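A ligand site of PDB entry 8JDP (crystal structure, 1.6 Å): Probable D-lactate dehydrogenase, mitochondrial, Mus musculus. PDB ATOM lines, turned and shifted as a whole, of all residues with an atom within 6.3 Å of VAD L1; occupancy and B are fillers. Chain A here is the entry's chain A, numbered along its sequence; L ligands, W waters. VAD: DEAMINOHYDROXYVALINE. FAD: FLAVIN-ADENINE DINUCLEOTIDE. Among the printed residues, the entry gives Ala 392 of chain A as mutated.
An oxygen (OE) of VAD L1 sits at hydrogen-bond distance from a ring nitrogen (NE2) of His 430, at 2.6 Å.
NH1 of Arg 334 lies within salt-bridge range of OXT of VAD L1 (2.7 Å).
OE1 of Glu 429 sits at hydrogen-bond distance from OE of VAD L1, 3.4 Å away.
N3 of FAD L2 sits at hydrogen-bond distance from OE2 of Glu 429.
NE2 of His 385 lies within hydrogen-bond range of O4 of FAD L2, at 3.1 Å.
N of Gly 146 is in hydrogen-bond range of N5 of FAD L2, 3.1 Å away.
N of His 430 lies within hydrogen-bond range of OD2 of Asp 354 (2.7 Å).
The guanidinium group of Arg 334 is in salt-bridge range of the side-chain carboxylate of Glu 264 (2.8 Å).
OE1 of Glu 429 is in hydrogen-bond range of NE2 of His 385, 3.1 Å away.
The backbone NH (N) of Glu 429 is in hydrogen-bond range of the side-chain carboxylate (OD2) of Asp 354 (2.8 Å).
N of Ala 392 is in hydrogen-bond range of O of Val 383 (2.7 Å).
The side-chain carboxylate (OE2) of Glu 264 lies within hydrogen-bond range of a ring nitrogen (ND1) of His 385 (2.7 Å).
Water W3 lies within hydrogen-bond range of an oxygen (OXT) of VAD L1, the backbone NH of Trp 338, the backbone carbonyl oxygen of His 335 and the backbone NH of Ala 337.
Water W1 lies within hydrogen-bond range of OXT of VAD L1 (2.9 Å), N of Gly 146 (3.1 Å) and NH1 of Arg 334 (3.4 Å).
Water W2 lies within hydrogen-bond range of OD1 of Asp 354, OE1 of Glu 429, NE2 of His 430 and OE of VAD L1.
Merely in contact with VAD L1: Ala 392 (3.7 Å), His 385 (3.7 Å), Ser 352 (3.7 Å) and Trp 338 (3.7 Å).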
ATOM      1  N   VAL A  88       9.870  -5.853  18.253  1.00  0.00           N
ATOM      2  CA  VAL A  88       9.775  -6.604  19.503  1.00  0.00           C
ATOM      3  C   VAL A  88      11.123  -6.761  20.194  1.00  0.00           C
ATOM      4  O   VAL A  88      11.273  -7.614  21.082  1.00  0.00           O
ATOM      5  CB  VAL A  88       9.121  -7.982  19.261  1.00  0.00           C
ATOM      6  CG1 VAL A  88       7.664  -7.815  18.831  1.00  0.00           C
ATOM      7  CG2 VAL A  88       9.886  -8.769  18.215  1.00  0.00           C
ATOM      8  N   GLY A 146       2.726 -10.123  11.120  1.00  0.00           N
ATOM      9  CA  GLY A 146       1.357 -10.039  11.609  1.00  0.00           C
ATOM     10  C   GLY A 146       0.920  -8.622  11.937  1.00  0.00           C
ATOM     11  O   GLY A 146      -0.282  -8.324  11.938  1.00  0.00           O
ATOM     12  N   GLU A 264       2.695 -23.024   9.137  1.00  0.00           N
ATOM     13  CA  GLU A 264       2.846 -22.381  10.429  1.00  0.00           C
ATOM     14  C   GLU A 264       2.494 -23.359  11.538  1.00  0.00           C
ATOM     15  O   GLU A 264       1.515 -24.097  11.435  1.00  0.00           O
ATOM     16  CB  GLU A 264       1.934 -21.161  10.545  1.00  0.00           C
ATOM     17  CG  GLU A 264       2.329 -20.046   9.607  1.00  0.00           C
ATOM     18  CD  GLU A 264       3.618 -19.373  10.041  1.00  0.00           C
ATOM     19  OE1 GLU A 264       3.765 -19.126  11.239  1.00  0.00           O
ATOM     20  OE2 GLU A 264       4.478 -19.116   9.167  1.00  0.00           O
ATOM     21  N   ARG A 334      -3.797 -16.178  13.030  1.00  0.00           N
ATOM     22  CA  ARG A 334      -2.360 -16.429  13.105  1.00  0.00           C
ATOM     23  C   ARG A 334      -1.584 -15.125  13.247  1.00  0.00           C
ATOM     24  O   ARG A 334      -0.682 -15.012  14.076  1.00  0.00           O
ATOM     25  CB  ARG A 334      -1.901 -17.192  11.869  1.00  0.00           C
ATOM     26  CG  ARG A 334      -0.383 -17.235  11.673  1.00  0.00           C
ATOM     27  CD  ARG A 334       0.312 -17.937  12.824  1.00  0.00           C
ATOM     28  NE  ARG A 334       1.767 -17.840  12.702  1.00  0.00           N
ATOM     29  CZ  ARG A 334       2.505 -16.876  13.248  1.00  0.00           C
ATOM     30  NH1 ARG A 334       1.932 -15.929  13.974  1.00  0.00           N
ATOM     31  NH2 ARG A 334       3.824 -16.881  13.062  1.00  0.00           N
ATOM     32  N   HIS A 335      -1.938 -14.122  12.434  1.00  0.00           N
ATOM     33  CA  HIS A 335      -1.239 -12.848  12.474  1.00  0.00           C
ATOM     34  C   HIS A 335      -1.363 -12.159  13.824  1.00  0.00           C
ATOM     35  O   HIS A 335      -0.487 -11.369  14.190  1.00  0.00           O
ATOM     36  CB  HIS A 335      -1.761 -11.941  11.359  1.00  0.00           C
ATOM     37  CG  HIS A 335      -1.200 -12.256  10.006  1.00  0.00           C
ATOM     38  ND1 HIS A 335      -1.903 -12.044   8.843  1.00  0.00           N
ATOM     39  CD2 HIS A 335       0.008 -12.761   9.645  1.00  0.00           C
ATOM     40  CE1 HIS A 335      -1.149 -12.403   7.811  1.00  0.00           C
ATOM     41  NE2 HIS A 335       0.010 -12.842   8.274  1.00  0.00           N
ATOM     42  N   ASN A 336      -2.424 -12.444  14.584  1.00  0.00           N
ATOM     43  CA  ASN A 336      -2.637 -11.813  15.874  1.00  0.00           C
ATOM     44  C   ASN A 336      -2.219 -12.703  17.044  1.00  0.00           C
ATOM     45  O   ASN A 336      -2.524 -12.390  18.198  1.00  0.00           O
ATOM     46  CB  ASN A 336      -4.105 -11.403  16.019  1.00  0.00           C
ATOM     47  CG  ASN A 336      -4.396 -10.105  15.301  1.00  0.00           C
ATOM     48  OD1 ASN A 336      -3.960  -9.043  15.740  1.00  0.00           O
ATOM     49  ND2 ASN A 336      -5.117 -10.187  14.195  1.00  0.00           N
ATOM     50  N   ALA A 337      -1.469 -13.782  16.759  1.00  0.00           N
ATOM     51  CA  ALA A 337      -1.045 -14.717  17.808  1.00  0.00           C
ATOM     52  C   ALA A 337      -0.327 -14.002  18.950  1.00  0.00           C
ATOM     53  O   ALA A 337      -0.499 -14.355  20.121  1.00  0.00           O
ATOM     54  CB  ALA A 337      -0.148 -15.788  17.215  1.00  0.00           C
ATOM     55  N   TRP A 338       0.504 -13.001  18.637  1.00  0.00           N
ATOM     56  CA  TRP A 338       1.177 -12.241  19.683  1.00  0.00           C
ATOM     57  C   TRP A 338       0.172 -11.643  20.655  1.00  0.00           C
ATOM     58  O   TRP A 338       0.352 -11.728  21.882  1.00  0.00           O
ATOM     59  CB  TRP A 338       2.029 -11.151  19.032  1.00  0.00           C
ATOM     60  CG  TRP A 338       2.623 -10.135  19.967  1.00  0.00           C
ATOM     61  CD1 TRP A 338       2.164  -8.875  20.194  1.00  0.00           C
ATOM     62  CD2 TRP A 338       3.800 -10.289  20.755  1.00  0.00           C
ATOM     63  NE1 TRP A 338       2.991  -8.228  21.090  1.00  0.00           N
ATOM     64  CE2 TRP A 338       3.997  -9.079  21.443  1.00  0.00           C
ATOM     65  CE3 TRP A 338       4.703 -11.335  20.951  1.00  0.00           C
ATOM     66  CZ2 TRP A 338       5.060  -8.888  22.328  1.00  0.00           C
ATOM     67  CZ3 TRP A 338       5.759 -11.143  21.820  1.00  0.00           C
ATOM     68  CH2 TRP A 338       5.932  -9.929  22.495  1.00  0.00           C
ATOM     69  N   SER A 352       9.707 -12.368  23.202  1.00  0.00           N
ATOM     70  CA  SER A 352       9.681 -13.401  22.180  1.00  0.00           C
ATOM     71  C   SER A 352      11.093 -13.847  21.853  1.00  0.00           C
ATOM     72  O   SER A 352      11.973 -13.018  21.597  1.00  0.00           O
ATOM     73  CB  SER A 352       9.013 -12.911  20.901  1.00  0.00           C
ATOM     74  OG  SER A 352       8.733 -14.013  20.057  1.00  0.00           O
ATOM     75  N   THR A 353      11.314 -15.164  21.837  1.00  0.00           N
ATOM     76  CA  THR A 353      12.484 -15.702  21.178  1.00  0.00           C
ATOM     77  C   THR A 353      12.200 -15.843  19.690  1.00  0.00           C
ATOM     78  O   THR A 353      11.073 -15.672  19.231  1.00  0.00           O
ATOM     79  CB  THR A 353      12.879 -17.045  21.806  1.00  0.00           C
ATOM     80  OG1 THR A 353      11.858 -18.022  21.559  1.00  0.00           O
ATOM     81  CG2 THR A 353      13.073 -16.886  23.299  1.00  0.00           C
ATOM     82  N   ASP A 354      13.245 -16.169  18.918  1.00  0.00           N
ATOM     83  CA  ASP A 354      13.155 -16.129  17.467  1.00  0.00           C
ATOM     84  C   ASP A 354      14.227 -16.975  16.772  1.00  0.00           C
ATOM     85  O   ASP A 354      14.675 -16.623  15.680  1.00  0.00           O
ATOM     86  CB  ASP A 354      13.260 -14.675  16.985  1.00  0.00           C
ATOM     87  CG  ASP A 354      12.921 -14.504  15.514  1.00  0.00           C
ATOM     88  OD1 ASP A 354      12.049 -15.224  14.975  1.00  0.00           O
ATOM     89  OD2 ASP A 354      13.567 -13.639  14.889  1.00  0.00           O
ATOM     90  N   VAL A 383       4.766 -20.518  18.594  1.00  0.00           N
ATOM     91  CA  VAL A 383       4.233 -20.306  17.252  1.00  0.00           C
ATOM     92  C   VAL A 383       5.443 -20.092  16.361  1.00  0.00           C
ATOM     93  O   VAL A 383       6.464 -19.557  16.795  1.00  0.00           O
ATOM     94  CB  VAL A 383       3.257 -19.108  17.205  1.00  0.00           C
ATOM     95  CG1 VAL A 383       3.994 -17.780  17.405  1.00  0.00           C
ATOM     96  CG2 VAL A 383       2.470 -19.109  15.908  1.00  0.00           C
ATOM     97  N   GLY A 384       5.370 -20.553  15.109  1.00  0.00           N
ATOM     98  CA  GLY A 384       6.586 -20.508  14.320  1.00  0.00           C
ATOM     99  C   GLY A 384       6.398 -20.625  12.829  1.00  0.00           C
ATOM    100  O   GLY A 384       5.577 -21.403  12.344  1.00  0.00           O
ATOM    101  N   HIS A 385       7.221 -19.863  12.102  1.00  0.00           N
ATOM    102  CA  HIS A 385       7.450 -20.048  10.669  1.00  0.00           C
ATOM    103  C   HIS A 385       8.368 -21.258  10.474  1.00  0.00           C
ATOM    104  O   HIS A 385       9.527 -21.149  10.054  1.00  0.00           O
ATOM    105  CB  HIS A 385       8.102 -18.806  10.059  1.00  0.00           C
ATOM    106  CG  HIS A 385       7.438 -17.513  10.421  1.00  0.00           C
ATOM    107  ND1 HIS A 385       6.105 -17.252  10.140  1.00  0.00           N
ATOM    108  CD2 HIS A 385       7.934 -16.384  10.984  1.00  0.00           C
ATOM    109  CE1 HIS A 385       5.815 -16.027  10.535  1.00  0.00           C
ATOM    110  NE2 HIS A 385       6.905 -15.468  11.043  1.00  0.00           N
ATOM    111  N   ALA A 392       9.007 -19.004  17.426  1.00  0.00           N
ATOM    112  CA  ALA A 392       9.012 -18.057  18.520  1.00  0.00           C
ATOM    113  C   ALA A 392       8.420 -18.696  19.758  1.00  0.00           C
ATOM    114  O   ALA A 392       7.412 -19.404  19.683  1.00  0.00           O
ATOM    115  CB  ALA A 392       8.218 -16.790  18.161  1.00  0.00           C
ATOM    116  N   ILE A 394       6.761 -17.269  23.052  1.00  0.00           N
ATOM    117  CA  ILE A 394       6.219 -16.033  23.601  1.00  0.00           C
ATOM    118  C   ILE A 394       6.067 -16.224  25.103  1.00  0.00           C
ATOM    119  O   ILE A 394       5.269 -17.049  25.545  1.00  0.00           O
ATOM    120  CB  ILE A 394       4.871 -15.664  22.962  1.00  0.00           C
ATOM    121  CG1 ILE A 394       5.014 -15.485  21.445  1.00  0.00           C
ATOM    122  CG2 ILE A 394       4.330 -14.397  23.615  1.00  0.00           C
ATOM    123  CD1 ILE A 394       3.674 -15.435  20.727  1.00  0.00           C
ATOM    124  N   GLU A 429      14.214 -13.397  12.194  1.00  0.00           N
ATOM    125  CA  GLU A 429      13.527 -12.282  11.544  1.00  0.00           C
ATOM    126  C   GLU A 429      13.370 -11.034  12.396  1.00  0.00           C
ATOM    127  O   GLU A 429      13.318  -9.923  11.857  1.00  0.00           O
ATOM    128  CB  GLU A 429      12.157 -12.756  11.044  1.00  0.00           C
ATOM    129  CG  GLU A 429      11.336 -13.475  12.118  1.00  0.00           C
ATOM    130  CD  GLU A 429       9.880 -13.630  11.733  1.00  0.00           C
ATOM    131  OE1 GLU A 429       9.021 -13.810  12.640  1.00  0.00           O
ATOM    132  OE2 GLU A 429       9.568 -13.586  10.523  1.00  0.00           O
ATOM    133  N   HIS A 430      13.292 -11.170  13.729  1.00  0.00           N
ATOM    134  CA  HIS A 430      12.965 -10.015  14.567  1.00  0.00           C
ATOM    135  C   HIS A 430      14.116  -9.036  14.705  1.00  0.00           C
ATOM    136  O   HIS A 430      13.898  -7.833  14.899  1.00  0.00           O
ATOM    137  CB  HIS A 430      12.562 -10.478  15.966  1.00  0.00           C
ATOM    138  CG  HIS A 430      11.261 -11.197  16.023  1.00  0.00           C
ATOM    139  ND1 HIS A 430      10.920 -12.031  17.065  1.00  0.00           N
ATOM    140  CD2 HIS A 430      10.215 -11.213  15.166  1.00  0.00           C
ATOM    141  CE1 HIS A 430       9.729 -12.539  16.844  1.00  0.00           C
ATOM    142  NE2 HIS A 430       9.266 -12.058  15.707  1.00  0.00           N
HETATM  143  CA  VAD L   1       5.576 -12.806  15.425  1.00  0.00           C
HETATM  144  CB  VAD L   1       5.347 -12.730  16.930  1.00  0.00           C
HETATM  145  CG1 VAD L   1       6.057 -11.498  17.464  1.00  0.00           C
HETATM  146  CG2 VAD L   1       5.921 -13.975  17.601  1.00  0.00           C
HETATM  147  C   VAD L   1       4.739 -13.919  14.827  1.00  0.00           C
HETATM  148  O   VAD L   1       5.314 -14.925  14.323  1.00  0.00           O
HETATM  149  OXT VAD L   1       3.482 -13.844  14.838  1.00  0.00           O
HETATM  150  OE  VAD L   1       6.928 -13.054  15.151  1.00  0.00           O
HETATM  151  PA  FAD L   2       9.886  -0.067  14.535  1.00  0.00           P
HETATM  152  O1A FAD L   2       9.621  -0.749  15.824  1.00  0.00           O
HETATM  153  O2A FAD L   2       9.359   1.321  14.257  1.00  0.00           O
HETATM  154  O5B FAD L   2      11.433  -0.057  14.330  1.00  0.00           O
HETATM  155  C5B FAD L   2      12.197  -1.287  14.394  1.00  0.00           C
HETATM  156  C4B FAD L   2      13.673  -1.027  14.233  1.00  0.00           C
HETATM  157  O4B FAD L   2      13.958  -0.609  12.883  1.00  0.00           O
HETATM  158  C3B FAD L   2      14.259   0.048  15.139  1.00  0.00           C
HETATM  159  O3B FAD L   2      15.608  -0.259  15.465  1.00  0.00           O
HETATM  160  C2B FAD L   2      14.130   1.304  14.274  1.00  0.00           C
HETATM  161  O2B FAD L   2      15.091   2.299  14.601  1.00  0.00           O
HETATM  162  C1B FAD L   2      14.399   0.741  12.876  1.00  0.00           C
HETATM  163  N9A FAD L   2      13.724   1.417  11.784  1.00  0.00           N
HETATM  164  C8A FAD L   2      12.368   1.528  11.575  1.00  0.00           C
HETATM  165  N7A FAD L   2      12.049   2.167  10.470  1.00  0.00           N
HETATM  166  C5A FAD L   2      13.282   2.466   9.902  1.00  0.00           C
HETATM  167  C6A FAD L   2      13.635   3.133   8.710  1.00  0.00           C
HETATM  168  N6A FAD L   2      12.754   3.625   7.840  1.00  0.00           N
HETATM  169  N1A FAD L   2      14.956   3.259   8.441  1.00  0.00           N
HETATM  170  C2A FAD L   2      15.843   2.767   9.303  1.00  0.00           C
HETATM  171  N3A FAD L   2      15.620   2.114  10.443  1.00  0.00           N
HETATM  172  C4A FAD L   2      14.316   2.001  10.686  1.00  0.00           C
HETATM  173  N1  FAD L   2       8.385  -9.454  12.460  1.00  0.00           N
HETATM  174  C2  FAD L   2       8.748 -10.381  11.532  1.00  0.00           C
HETATM  175  O2  FAD L   2       9.862 -10.354  10.985  1.00  0.00           O
HETATM  176  N3  FAD L   2       7.859 -11.392  11.177  1.00  0.00           N
HETATM  177  C4  FAD L   2       6.585 -11.554  11.683  1.00  0.00           C
HETATM  178  O4  FAD L   2       5.887 -12.501  11.298  1.00  0.00           O
HETATM  179  C4X FAD L   2       6.200 -10.555  12.666  1.00  0.00           C
HETATM  180  N5  FAD L   2       4.991 -10.627  13.194  1.00  0.00           N
HETATM  181  C5X FAD L   2       4.632  -9.679  14.135  1.00  0.00           C
HETATM  182  C6  FAD L   2       3.369  -9.746  14.702  1.00  0.00           C
HETATM  183  C7  FAD L   2       2.956  -8.806  15.647  1.00  0.00           C
HETATM  184  C7M FAD L   2       1.568  -8.916  16.247  1.00  0.00           C
HETATM  185  C8  FAD L   2       3.832  -7.789  16.041  1.00  0.00           C
HETATM  186  C8M FAD L   2       3.421  -6.752  17.064  1.00  0.00           C
HETATM  187  C9  FAD L   2       5.095  -7.714  15.462  1.00  0.00           C
HETATM  188  C9A FAD L   2       5.503  -8.654  14.525  1.00  0.00           C
HETATM  189  N10 FAD L   2       6.779  -8.587  13.908  1.00  0.00           N
HETATM  190  C10 FAD L   2       7.163  -9.546  12.993  1.00  0.00           C
HETATM  191  C1' FAD L   2       7.767  -7.584  14.332  1.00  0.00           C
HETATM  192  C2' FAD L   2       7.662  -6.238  13.617  1.00  0.00           C
HETATM  193  O2' FAD L   2       6.343  -6.035  13.115  1.00  0.00           O
HETATM  194  C3' FAD L   2       8.694  -6.199  12.491  1.00  0.00           C
HETATM  195  O3' FAD L   2       9.989  -6.282  13.079  1.00  0.00           O
HETATM  196  C4' FAD L   2       8.593  -4.927  11.653  1.00  0.00           C
HETATM  197  O4' FAD L   2       9.523  -5.041  10.565  1.00  0.00           O
HETATM  198  C5' FAD L   2       8.891  -3.698  12.469  1.00  0.00           C
HETATM  199  O5' FAD L   2       8.595  -2.525  11.672  1.00  0.00           O
HETATM  200  P   FAD L   2       8.262  -1.157  12.361  1.00  0.00           P
HETATM  201  O1P FAD L   2       8.315  -0.011  11.339  1.00  0.00           O
HETATM  202  O2P FAD L   2       7.020  -1.271  13.149  1.00  0.00           O
HETATM  203  O3P FAD L   2       9.506  -1.028  13.330  1.00  0.00           O
HETATM  204  O   HOH W   1       2.417 -13.046  12.234  1.00  0.00           O
HETATM  205  O   HOH W   2       9.503 -15.309  14.779  1.00  0.00           O
HETATM  206  O   HOH W   3       1.489 -12.506  16.048  1.00  0.00           O
